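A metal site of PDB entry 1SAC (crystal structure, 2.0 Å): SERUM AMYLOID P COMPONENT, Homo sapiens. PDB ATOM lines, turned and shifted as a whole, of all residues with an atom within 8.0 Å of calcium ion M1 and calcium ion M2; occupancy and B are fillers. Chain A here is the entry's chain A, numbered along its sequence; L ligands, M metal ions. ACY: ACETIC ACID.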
ATOM      1  N   SER A  48     -16.312 -31.006   5.550  1.00  0.00           N
ATOM      2  CA  SER A  48     -15.699 -30.143   6.573  1.00  0.00           C
ATOM      3  C   SER A  48     -16.329 -30.413   7.933  1.00  0.00           C
ATOM      4  O   SER A  48     -17.557 -30.479   8.027  1.00  0.00           O
ATOM      5  CB  SER A  48     -15.920 -28.677   6.188  1.00  0.00           C
ATOM      6  OG  SER A  48     -15.155 -27.827   7.032  1.00  0.00           O
ATOM      7  N   SER A  51     -14.378 -25.199  10.245  1.00  0.00           N
ATOM      8  CA  SER A  51     -13.822 -24.230   9.297  1.00  0.00           C
ATOM      9  C   SER A  51     -13.470 -22.929  10.037  1.00  0.00           C
ATOM     10  O   SER A  51     -14.363 -22.263  10.595  1.00  0.00           O
ATOM     11  CB  SER A  51     -14.830 -23.946   8.194  1.00  0.00           C
ATOM     12  OG  SER A  51     -14.223 -23.186   7.166  1.00  0.00           O
ATOM     13  N   TYR A  52     -12.192 -22.628   9.996  1.00  0.00           N
ATOM     14  CA  TYR A  52     -11.556 -21.493  10.689  1.00  0.00           C
ATOM     15  C   TYR A  52     -10.712 -20.683   9.686  1.00  0.00           C
ATOM     16  O   TYR A  52      -9.548 -21.030   9.412  1.00  0.00           O
ATOM     17  CB  TYR A  52     -10.681 -22.087  11.803  1.00  0.00           C
ATOM     18  CG  TYR A  52      -9.932 -21.080  12.678  1.00  0.00           C
ATOM     19  CD1 TYR A  52      -9.030 -20.174  12.093  1.00  0.00           C
ATOM     20  CD2 TYR A  52     -10.129 -21.081  14.066  1.00  0.00           C
ATOM     21  CE1 TYR A  52      -8.326 -19.269  12.911  1.00  0.00           C
ATOM     22  CE2 TYR A  52      -9.426 -20.176  14.869  1.00  0.00           C
ATOM     23  CZ  TYR A  52      -8.524 -19.270  14.299  1.00  0.00           C
ATOM     24  OH  TYR A  52      -7.833 -18.401  15.083  1.00  0.00           O
ATOM     25  N   ASN A  53     -11.317 -19.628   9.163  1.00  0.00           N
ATOM     26  CA  ASN A  53     -10.683 -18.738   8.177  1.00  0.00           C
ATOM     27  C   ASN A  53     -10.415 -17.357   8.793  1.00  0.00           C
ATOM     28  O   ASN A  53     -11.161 -16.885   9.645  1.00  0.00           O
ATOM     29  CB  ASN A  53     -11.605 -18.554   6.960  1.00  0.00           C
ATOM     30  CG  ASN A  53     -11.369 -19.617   5.869  1.00  0.00           C
ATOM     31  OD1 ASN A  53     -10.923 -20.719   6.177  1.00  0.00           O
ATOM     32  ND2 ASN A  53     -11.650 -19.332   4.608  1.00  0.00           N
ATOM     33  N   ARG A  57      -7.029 -15.282   4.417  1.00  0.00           N
ATOM     34  CA  ARG A  57      -6.377 -16.590   4.599  1.00  0.00           C
ATOM     35  C   ARG A  57      -7.385 -17.714   4.623  1.00  0.00           C
ATOM     36  O   ARG A  57      -8.094 -17.901   5.596  1.00  0.00           O
ATOM     37  CB  ARG A  57      -5.553 -16.602   5.887  1.00  0.00           C
ATOM     38  CG  ARG A  57      -4.152 -16.098   5.576  1.00  0.00           C
ATOM     39  CD  ARG A  57      -3.668 -15.162   6.675  1.00  0.00           C
ATOM     40  NE  ARG A  57      -2.447 -15.727   7.264  1.00  0.00           N
ATOM     41  CZ  ARG A  57      -1.407 -14.959   7.625  1.00  0.00           C
ATOM     42  NH1 ARG A  57      -1.323 -13.686   7.235  1.00  0.00           N
ATOM     43  NH2 ARG A  57      -0.450 -15.481   8.391  1.00  0.00           N
ATOM     44  N   ASP A  58      -7.420 -18.444   3.538  1.00  0.00           N
ATOM     45  CA  ASP A  58      -8.271 -19.653   3.478  1.00  0.00           C
ATOM     46  C   ASP A  58      -7.600 -20.803   4.213  1.00  0.00           C
ATOM     47  O   ASP A  58      -6.381 -20.867   4.231  1.00  0.00           O
ATOM     48  CB  ASP A  58      -8.463 -20.054   2.008  1.00  0.00           C
ATOM     49  CG  ASP A  58      -9.534 -21.139   1.901  1.00  0.00           C
ATOM     50  OD1 ASP A  58     -10.424 -21.139   2.772  1.00  0.00           O
ATOM     51  OD2 ASP A  58      -9.464 -21.936   0.960  1.00  0.00           O
ATOM     52  N   ASN A  59      -8.351 -21.650   4.871  1.00  0.00           N
ATOM     53  CA  ASN A  59      -7.823 -22.898   5.428  1.00  0.00           C
ATOM     54  C   ASN A  59      -6.716 -22.592   6.432  1.00  0.00           C
ATOM     55  O   ASN A  59      -5.668 -23.257   6.439  1.00  0.00           O
ATOM     56  CB  ASN A  59      -7.271 -23.772   4.303  1.00  0.00           C
ATOM     57  CG  ASN A  59      -8.406 -24.311   3.444  1.00  0.00           C
ATOM     58  OD1 ASN A  59      -9.569 -24.055   3.756  1.00  0.00           O
ATOM     59  ND2 ASN A  59      -8.140 -25.042   2.389  1.00  0.00           N
ATOM     60  N   GLU A  60      -7.049 -21.696   7.286  1.00  0.00           N
ATOM     61  CA  GLU A  60      -6.143 -21.244   8.348  1.00  0.00           C
ATOM     62  C   GLU A  60      -6.036 -22.326   9.450  1.00  0.00           C
ATOM     63  O   GLU A  60      -4.966 -22.573  10.008  1.00  0.00           O
ATOM     64  CB  GLU A  60      -6.656 -19.935   8.951  1.00  0.00           C
ATOM     65  CG  GLU A  60      -5.686 -19.310   9.946  1.00  0.00           C
ATOM     66  CD  GLU A  60      -4.314 -19.014   9.346  1.00  0.00           C
ATOM     67  OE1 GLU A  60      -4.093 -19.221   8.092  1.00  0.00           O
ATOM     68  OE2 GLU A  60      -3.368 -18.554  10.086  1.00  0.00           O
ATOM     69  N   LEU A  62      -8.463 -25.886   9.564  1.00  0.00           N
ATOM     70  CA  LEU A  62      -9.584 -26.675   9.002  1.00  0.00           C
ATOM     71  C   LEU A  62      -9.424 -28.155   9.335  1.00  0.00           C
ATOM     72  O   LEU A  62      -8.356 -28.741   9.118  1.00  0.00           O
ATOM     73  CB  LEU A  62      -9.610 -26.477   7.473  1.00  0.00           C
ATOM     74  CG  LEU A  62     -10.449 -27.518   6.718  1.00  0.00           C
ATOM     75  CD1 LEU A  62     -11.955 -27.340   6.934  1.00  0.00           C
ATOM     76  CD2 LEU A  62     -10.237 -27.468   5.200  1.00  0.00           C
ATOM     77  N   TYR A  64     -10.899 -31.667   8.402  1.00  0.00           N
ATOM     78  CA  TYR A  64     -11.586 -32.140   7.171  1.00  0.00           C
ATOM     79  C   TYR A  64     -11.608 -33.677   7.191  1.00  0.00           C
ATOM     80  O   TYR A  64     -10.585 -34.226   7.621  1.00  0.00           O
ATOM     81  CB  TYR A  64     -10.835 -31.659   5.959  1.00  0.00           C
ATOM     82  CG  TYR A  64     -11.616 -31.727   4.656  1.00  0.00           C
ATOM     83  CD1 TYR A  64     -12.611 -30.785   4.388  1.00  0.00           C
ATOM     84  CD2 TYR A  64     -11.322 -32.713   3.729  1.00  0.00           C
ATOM     85  CE1 TYR A  64     -13.316 -30.853   3.187  1.00  0.00           C
ATOM     86  CE2 TYR A  64     -12.022 -32.775   2.535  1.00  0.00           C
ATOM     87  CZ  TYR A  64     -13.026 -31.846   2.253  1.00  0.00           C
ATOM     88  OH  TYR A  64     -13.735 -31.885   1.073  1.00  0.00           O
ATOM     89  N   TYR A  74      -5.584 -28.903   8.481  1.00  0.00           N
ATOM     90  CA  TYR A  74      -4.910 -27.807   7.763  1.00  0.00           C
ATOM     91  C   TYR A  74      -4.508 -26.698   8.741  1.00  0.00           C
ATOM     92  O   TYR A  74      -5.330 -26.191   9.505  1.00  0.00           O
ATOM     93  CB  TYR A  74      -5.854 -27.107   6.777  1.00  0.00           C
ATOM     94  CG  TYR A  74      -6.140 -27.858   5.467  1.00  0.00           C
ATOM     95  CD1 TYR A  74      -7.019 -28.950   5.468  1.00  0.00           C
ATOM     96  CD2 TYR A  74      -5.533 -27.451   4.266  1.00  0.00           C
ATOM     97  CE1 TYR A  74      -7.304 -29.617   4.276  1.00  0.00           C
ATOM     98  CE2 TYR A  74      -5.831 -28.118   3.067  1.00  0.00           C
ATOM     99  CZ  TYR A  74      -6.714 -29.198   3.076  1.00  0.00           C
ATOM    100  OH  TYR A  74      -7.015 -29.836   1.912  1.00  0.00           O
ATOM    101  N   ARG A  77      -2.848 -23.481   5.632  1.00  0.00           N
ATOM    102  CA  ARG A  77      -2.971 -23.982   4.239  1.00  0.00           C
ATOM    103  C   ARG A  77      -2.111 -25.240   3.981  1.00  0.00           C
ATOM    104  O   ARG A  77      -2.162 -25.832   2.899  1.00  0.00           O
ATOM    105  CB  ARG A  77      -2.551 -22.908   3.253  1.00  0.00           C
ATOM    106  CG  ARG A  77      -3.723 -22.024   2.821  1.00  0.00           C
ATOM    107  CD  ARG A  77      -3.326 -20.562   2.610  1.00  0.00           C
ATOM    108  NE  ARG A  77      -2.447 -20.042   3.671  1.00  0.00           N
ATOM    109  CZ  ARG A  77      -2.864 -19.748   4.914  1.00  0.00           C
ATOM    110  NH1 ARG A  77      -4.141 -19.922   5.276  1.00  0.00           N
ATOM    111  NH2 ARG A  77      -2.063 -19.269   5.882  1.00  0.00           N
ATOM    112  N   GLN A 135     -20.654 -25.809   6.853  1.00  0.00           N
ATOM    113  CA  GLN A 135     -20.047 -25.538   5.537  1.00  0.00           C
ATOM    114  C   GLN A 135     -18.541 -25.322   5.697  1.00  0.00           C
ATOM    115  O   GLN A 135     -18.064 -24.993   6.790  1.00  0.00           O
ATOM    116  CB  GLN A 135     -20.660 -24.272   4.928  1.00  0.00           C
ATOM    117  CG  GLN A 135     -22.181 -24.317   4.862  1.00  0.00           C
ATOM    118  CD  GLN A 135     -22.718 -25.300   3.810  1.00  0.00           C
ATOM    119  OE1 GLN A 135     -22.011 -25.643   2.864  1.00  0.00           O
ATOM    120  NE2 GLN A 135     -23.944 -25.781   3.926  1.00  0.00           N
ATOM    121  N   GLU A 136     -17.943 -25.347   4.540  1.00  0.00           N
ATOM    122  CA  GLU A 136     -16.520 -25.070   4.334  1.00  0.00           C
ATOM    123  C   GLU A 136     -16.351 -23.706   3.652  1.00  0.00           C
ATOM    124  O   GLU A 136     -16.967 -23.431   2.604  1.00  0.00           O
ATOM    125  CB  GLU A 136     -15.912 -26.166   3.470  1.00  0.00           C
ATOM    126  CG  GLU A 136     -14.470 -26.477   3.844  1.00  0.00           C
ATOM    127  CD  GLU A 136     -13.505 -25.489   3.217  1.00  0.00           C
ATOM    128  OE1 GLU A 136     -13.659 -25.159   1.981  1.00  0.00           O
ATOM    129  OE2 GLU A 136     -12.547 -24.990   3.912  1.00  0.00           O
ATOM    130  N   GLN A 137     -15.626 -22.812   4.284  1.00  0.00           N
ATOM    131  CA  GLN A 137     -15.358 -21.455   3.802  1.00  0.00           C
ATOM    132  C   GLN A 137     -14.173 -21.402   2.839  1.00  0.00           C
ATOM    133  O   GLN A 137     -13.149 -22.062   3.053  1.00  0.00           O
ATOM    134  CB  GLN A 137     -14.916 -20.531   4.940  1.00  0.00           C
ATOM    135  CG  GLN A 137     -15.893 -20.409   6.103  1.00  0.00           C
ATOM    136  CD  GLN A 137     -15.307 -19.594   7.264  1.00  0.00           C
ATOM    137  OE1 GLN A 137     -15.244 -18.370   7.175  1.00  0.00           O
ATOM    138  NE2 GLN A 137     -14.864 -20.203   8.342  1.00  0.00           N
ATOM    139  N   ASP A 138     -14.355 -20.635   1.761  1.00  0.00           N
ATOM    140  CA  ASP A 138     -13.256 -20.335   0.837  1.00  0.00           C
ATOM    141  C   ASP A 138     -12.886 -18.857   0.933  1.00  0.00           C
ATOM    142  O   ASP A 138     -11.842 -18.430   0.427  1.00  0.00           O
ATOM    143  CB  ASP A 138     -13.669 -20.690  -0.592  1.00  0.00           C
ATOM    144  CG  ASP A 138     -13.324 -22.166  -0.824  1.00  0.00           C
ATOM    145  OD1 ASP A 138     -12.545 -22.779  -0.008  1.00  0.00           O
ATOM    146  OD2 ASP A 138     -13.812 -22.788  -1.849  1.00  0.00           O
ATOM    147  N   SER A 139     -13.770 -18.130   1.594  1.00  0.00           N
ATOM    148  CA  SER A 139     -13.598 -16.689   1.837  1.00  0.00           C
ATOM    149  C   SER A 139     -13.894 -16.390   3.299  1.00  0.00           C
ATOM    150  O   SER A 139     -14.075 -17.311   4.122  1.00  0.00           O
ATOM    151  CB  SER A 139     -14.543 -15.888   0.940  1.00  0.00           C
ATOM    152  OG  SER A 139     -15.893 -16.223   1.228  1.00  0.00           O
ATOM    153  N   GLY A 142     -17.517 -16.915   3.935  1.00  0.00           N
ATOM    154  CA  GLY A 142     -18.466 -17.361   2.897  1.00  0.00           C
ATOM    155  C   GLY A 142     -17.786 -18.285   1.887  1.00  0.00           C
ATOM    156  O   GLY A 142     -16.849 -18.977   2.263  1.00  0.00           O
ATOM    157  N   LYS A 143     -18.266 -18.249   0.668  1.00  0.00           N
ATOM    158  CA  LYS A 143     -17.849 -19.036  -0.479  1.00  0.00           C
ATOM    159  C   LYS A 143     -17.932 -20.520  -0.181  1.00  0.00           C
ATOM    160  O   LYS A 143     -16.942 -21.226  -0.325  1.00  0.00           O
ATOM    161  CB  LYS A 143     -16.457 -18.665  -0.934  1.00  0.00           C
ATOM    162  CG  LYS A 143     -16.515 -17.912  -2.247  1.00  0.00           C
ATOM    163  CD  LYS A 143     -15.415 -16.866  -2.289  1.00  0.00           C
ATOM    164  CE  LYS A 143     -14.124 -17.478  -2.809  1.00  0.00           C
ATOM    165  NZ  LYS A 143     -12.994 -16.566  -2.551  1.00  0.00           N
ATOM    166  N   PHE A 144     -19.063 -20.982   0.232  1.00  0.00           N
ATOM    167  CA  PHE A 144     -19.277 -22.380   0.628  1.00  0.00           C
ATOM    168  C   PHE A 144     -19.349 -23.263  -0.655  1.00  0.00           C
ATOM    169  O   PHE A 144     -19.525 -22.756  -1.768  1.00  0.00           O
ATOM    170  CB  PHE A 144     -20.585 -22.483   1.444  1.00  0.00           C
ATOM    171  CG  PHE A 144     -20.576 -21.602   2.710  1.00  0.00           C
ATOM    172  CD1 PHE A 144     -19.389 -21.430   3.438  1.00  0.00           C
ATOM    173  CD2 PHE A 144     -21.751 -20.956   3.137  1.00  0.00           C
ATOM    174  CE1 PHE A 144     -19.380 -20.635   4.586  1.00  0.00           C
ATOM    175  CE2 PHE A 144     -21.735 -20.149   4.285  1.00  0.00           C
ATOM    176  CZ  PHE A 144     -20.555 -19.989   5.013  1.00  0.00           C
ATOM    177  N   ASP A 145     -19.158 -24.580  -0.465  1.00  0.00           N
ATOM    178  CA  ASP A 145     -19.246 -25.607  -1.558  1.00  0.00           C
ATOM    179  C   ASP A 145     -20.099 -26.780  -1.059  1.00  0.00           C
ATOM    180  O   ASP A 145     -19.849 -27.320   0.036  1.00  0.00           O
ATOM    181  CB  ASP A 145     -17.833 -26.134  -1.919  1.00  0.00           C
ATOM    182  CG  ASP A 145     -17.776 -27.310  -2.938  1.00  0.00           C
ATOM    183  OD1 ASP A 145     -18.861 -27.851  -3.390  1.00  0.00           O
ATOM    184  OD2 ASP A 145     -16.635 -27.755  -3.348  1.00  0.00           O
ATOM    185  N   ARG A 146     -21.247 -26.901  -1.664  1.00  0.00           N
ATOM    186  CA  ARG A 146     -22.213 -27.943  -1.318  1.00  0.00           C
ATOM    187  C   ARG A 146     -21.570 -29.317  -1.190  1.00  0.00           C
ATOM    188  O   ARG A 146     -22.047 -30.174  -0.428  1.00  0.00           O
ATOM    189  CB  ARG A 146     -23.301 -28.019  -2.367  1.00  0.00           C
ATOM    190  CG  ARG A 146     -24.245 -29.168  -2.119  1.00  0.00           C
ATOM    191  CD  ARG A 146     -25.217 -29.336  -3.264  1.00  0.00           C
ATOM    192  NE  ARG A 146     -26.329 -28.410  -3.184  1.00  0.00           N
ATOM    193  CZ  ARG A 146     -27.497 -28.737  -2.660  1.00  0.00           C
ATOM    194  NH1 ARG A 146     -27.700 -29.976  -2.193  1.00  0.00           N
ATOM    195  NH2 ARG A 146     -28.527 -27.888  -2.561  1.00  0.00           N
ATOM    196  N   SER A 147     -20.553 -29.678  -1.915  1.00  0.00           N
ATOM    197  CA  SER A 147     -19.956 -31.026  -1.856  1.00  0.00           C
ATOM    198  C   SER A 147     -18.978 -31.124  -0.694  1.00  0.00           C
ATOM    199  O   SER A 147     -18.261 -32.100  -0.500  1.00  0.00           O
ATOM    200  CB  SER A 147     -19.241 -31.336  -3.173  1.00  0.00           C
ATOM    201  OG  SER A 147     -18.108 -30.470  -3.281  1.00  0.00           O
ATOM    202  N   GLN A 148     -18.972 -30.114   0.135  1.00  0.00           N
ATOM    203  CA  GLN A 148     -18.144 -30.186   1.340  1.00  0.00           C
ATOM    204  C   GLN A 148     -18.985 -29.936   2.582  1.00  0.00           C
ATOM    205  O   GLN A 148     -18.462 -29.738   3.691  1.00  0.00           O
ATOM    206  CB  GLN A 148     -17.058 -29.124   1.292  1.00  0.00           C
ATOM    207  CG  GLN A 148     -16.056 -29.337   0.151  1.00  0.00           C
ATOM    208  CD  GLN A 148     -14.877 -28.398   0.293  1.00  0.00           C
ATOM    209  OE1 GLN A 148     -15.060 -27.226   0.610  1.00  0.00           O
ATOM    210  NE2 GLN A 148     -13.651 -28.856   0.111  1.00  0.00           N
HETATM  211  C   ACY L   1     -11.077 -26.426   0.481  1.00  0.00           C
HETATM  212  O   ACY L   1     -10.406 -25.404   0.318  1.00  0.00           O
HETATM  213  OXT ACY L   1     -12.009 -26.644  -0.311  1.00  0.00           O
HETATM  214  CH3 ACY L   1     -10.468 -27.600   1.264  1.00  0.00           C
HETATM  215 CA    CA M   1     -11.388 -23.550   2.101  1.00  0.00          CA
HETATM  216 CA    CA M   2     -14.129 -25.021  -0.369  1.00  0.00          CA
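Of the 24 residues printed, 5 come within 4 Å of calcium ion M1. The nearest printed residue that does not touch calcium ion M1 is Asn 53 (4.9 Å).
O of Gln 137 is bound to calcium ion M1, 2.5 Å away. Calcium ion M1 is bound by OD1 of Asn 59 (2.5 Å). The side-chain carboxylate (OD1) of Asp 138 binds calcium ion M1 (2.5 Å). OE2 of Glu 136 is bound to calcium ion M1, 2.6 Å away. Calcium ion M1 is bound by OD1 of Asp 58. Calcium ion M1 is bound by O of the ligand (2.8 Å). OD2 of Asp 58 is bound to calcium ion M1 (2.8 Å). Calcium ion M1 is bound by OE1 of Glu 136 (2.8 Å).
Calcium ion M2 is bound by OE1 of Glu 136 (2.4 Å), OE1 of Gln 148 (2.6 Å), OXT of the ligand (2.7 Å), OD2 of Asp 138 (2.7 Å) and OD1 of Asp 138 (2.8 Å). Calcium ion M2 has five donor atoms within binding distance.
The backbone carbonyl oxygen of Asp 58 sits at hydrogen-bond distance from the guanidinium group of Arg 77 (2.6 Å). The backbone NH (N) of Asn 59 is in hydrogen-bond range of the side-chain amide oxygen (OD1) of Asn 53, at 3.0 Å. The backbone NH of Arg 77 is in hydrogen-bond range of the backbone carbonyl oxygen of Asn 59. OE1 of Gln 137 lies close to O of Ser 139, 3.4 Å away. OD1 of Asp 58 sits close to ND2 of Asn 53. The backbone carbonyl oxygen (O) of Gln 148 lies within hydrogen-bond range of the backbone NH (N) of Ser 48 (3.1 Å). NE2 of Gln 148 sits at hydrogen-bond distance from OH of Tyr 64 (3.2 Å). O of Lys 143 sits close to N of Asp 138, 3.4 Å away.
Within 4 Å of calcium ion M2: Glu 136, Asp 138 and Gln 148. Along chain A the residues within 4 Å of calcium ion M2 span positions 136 to 148.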
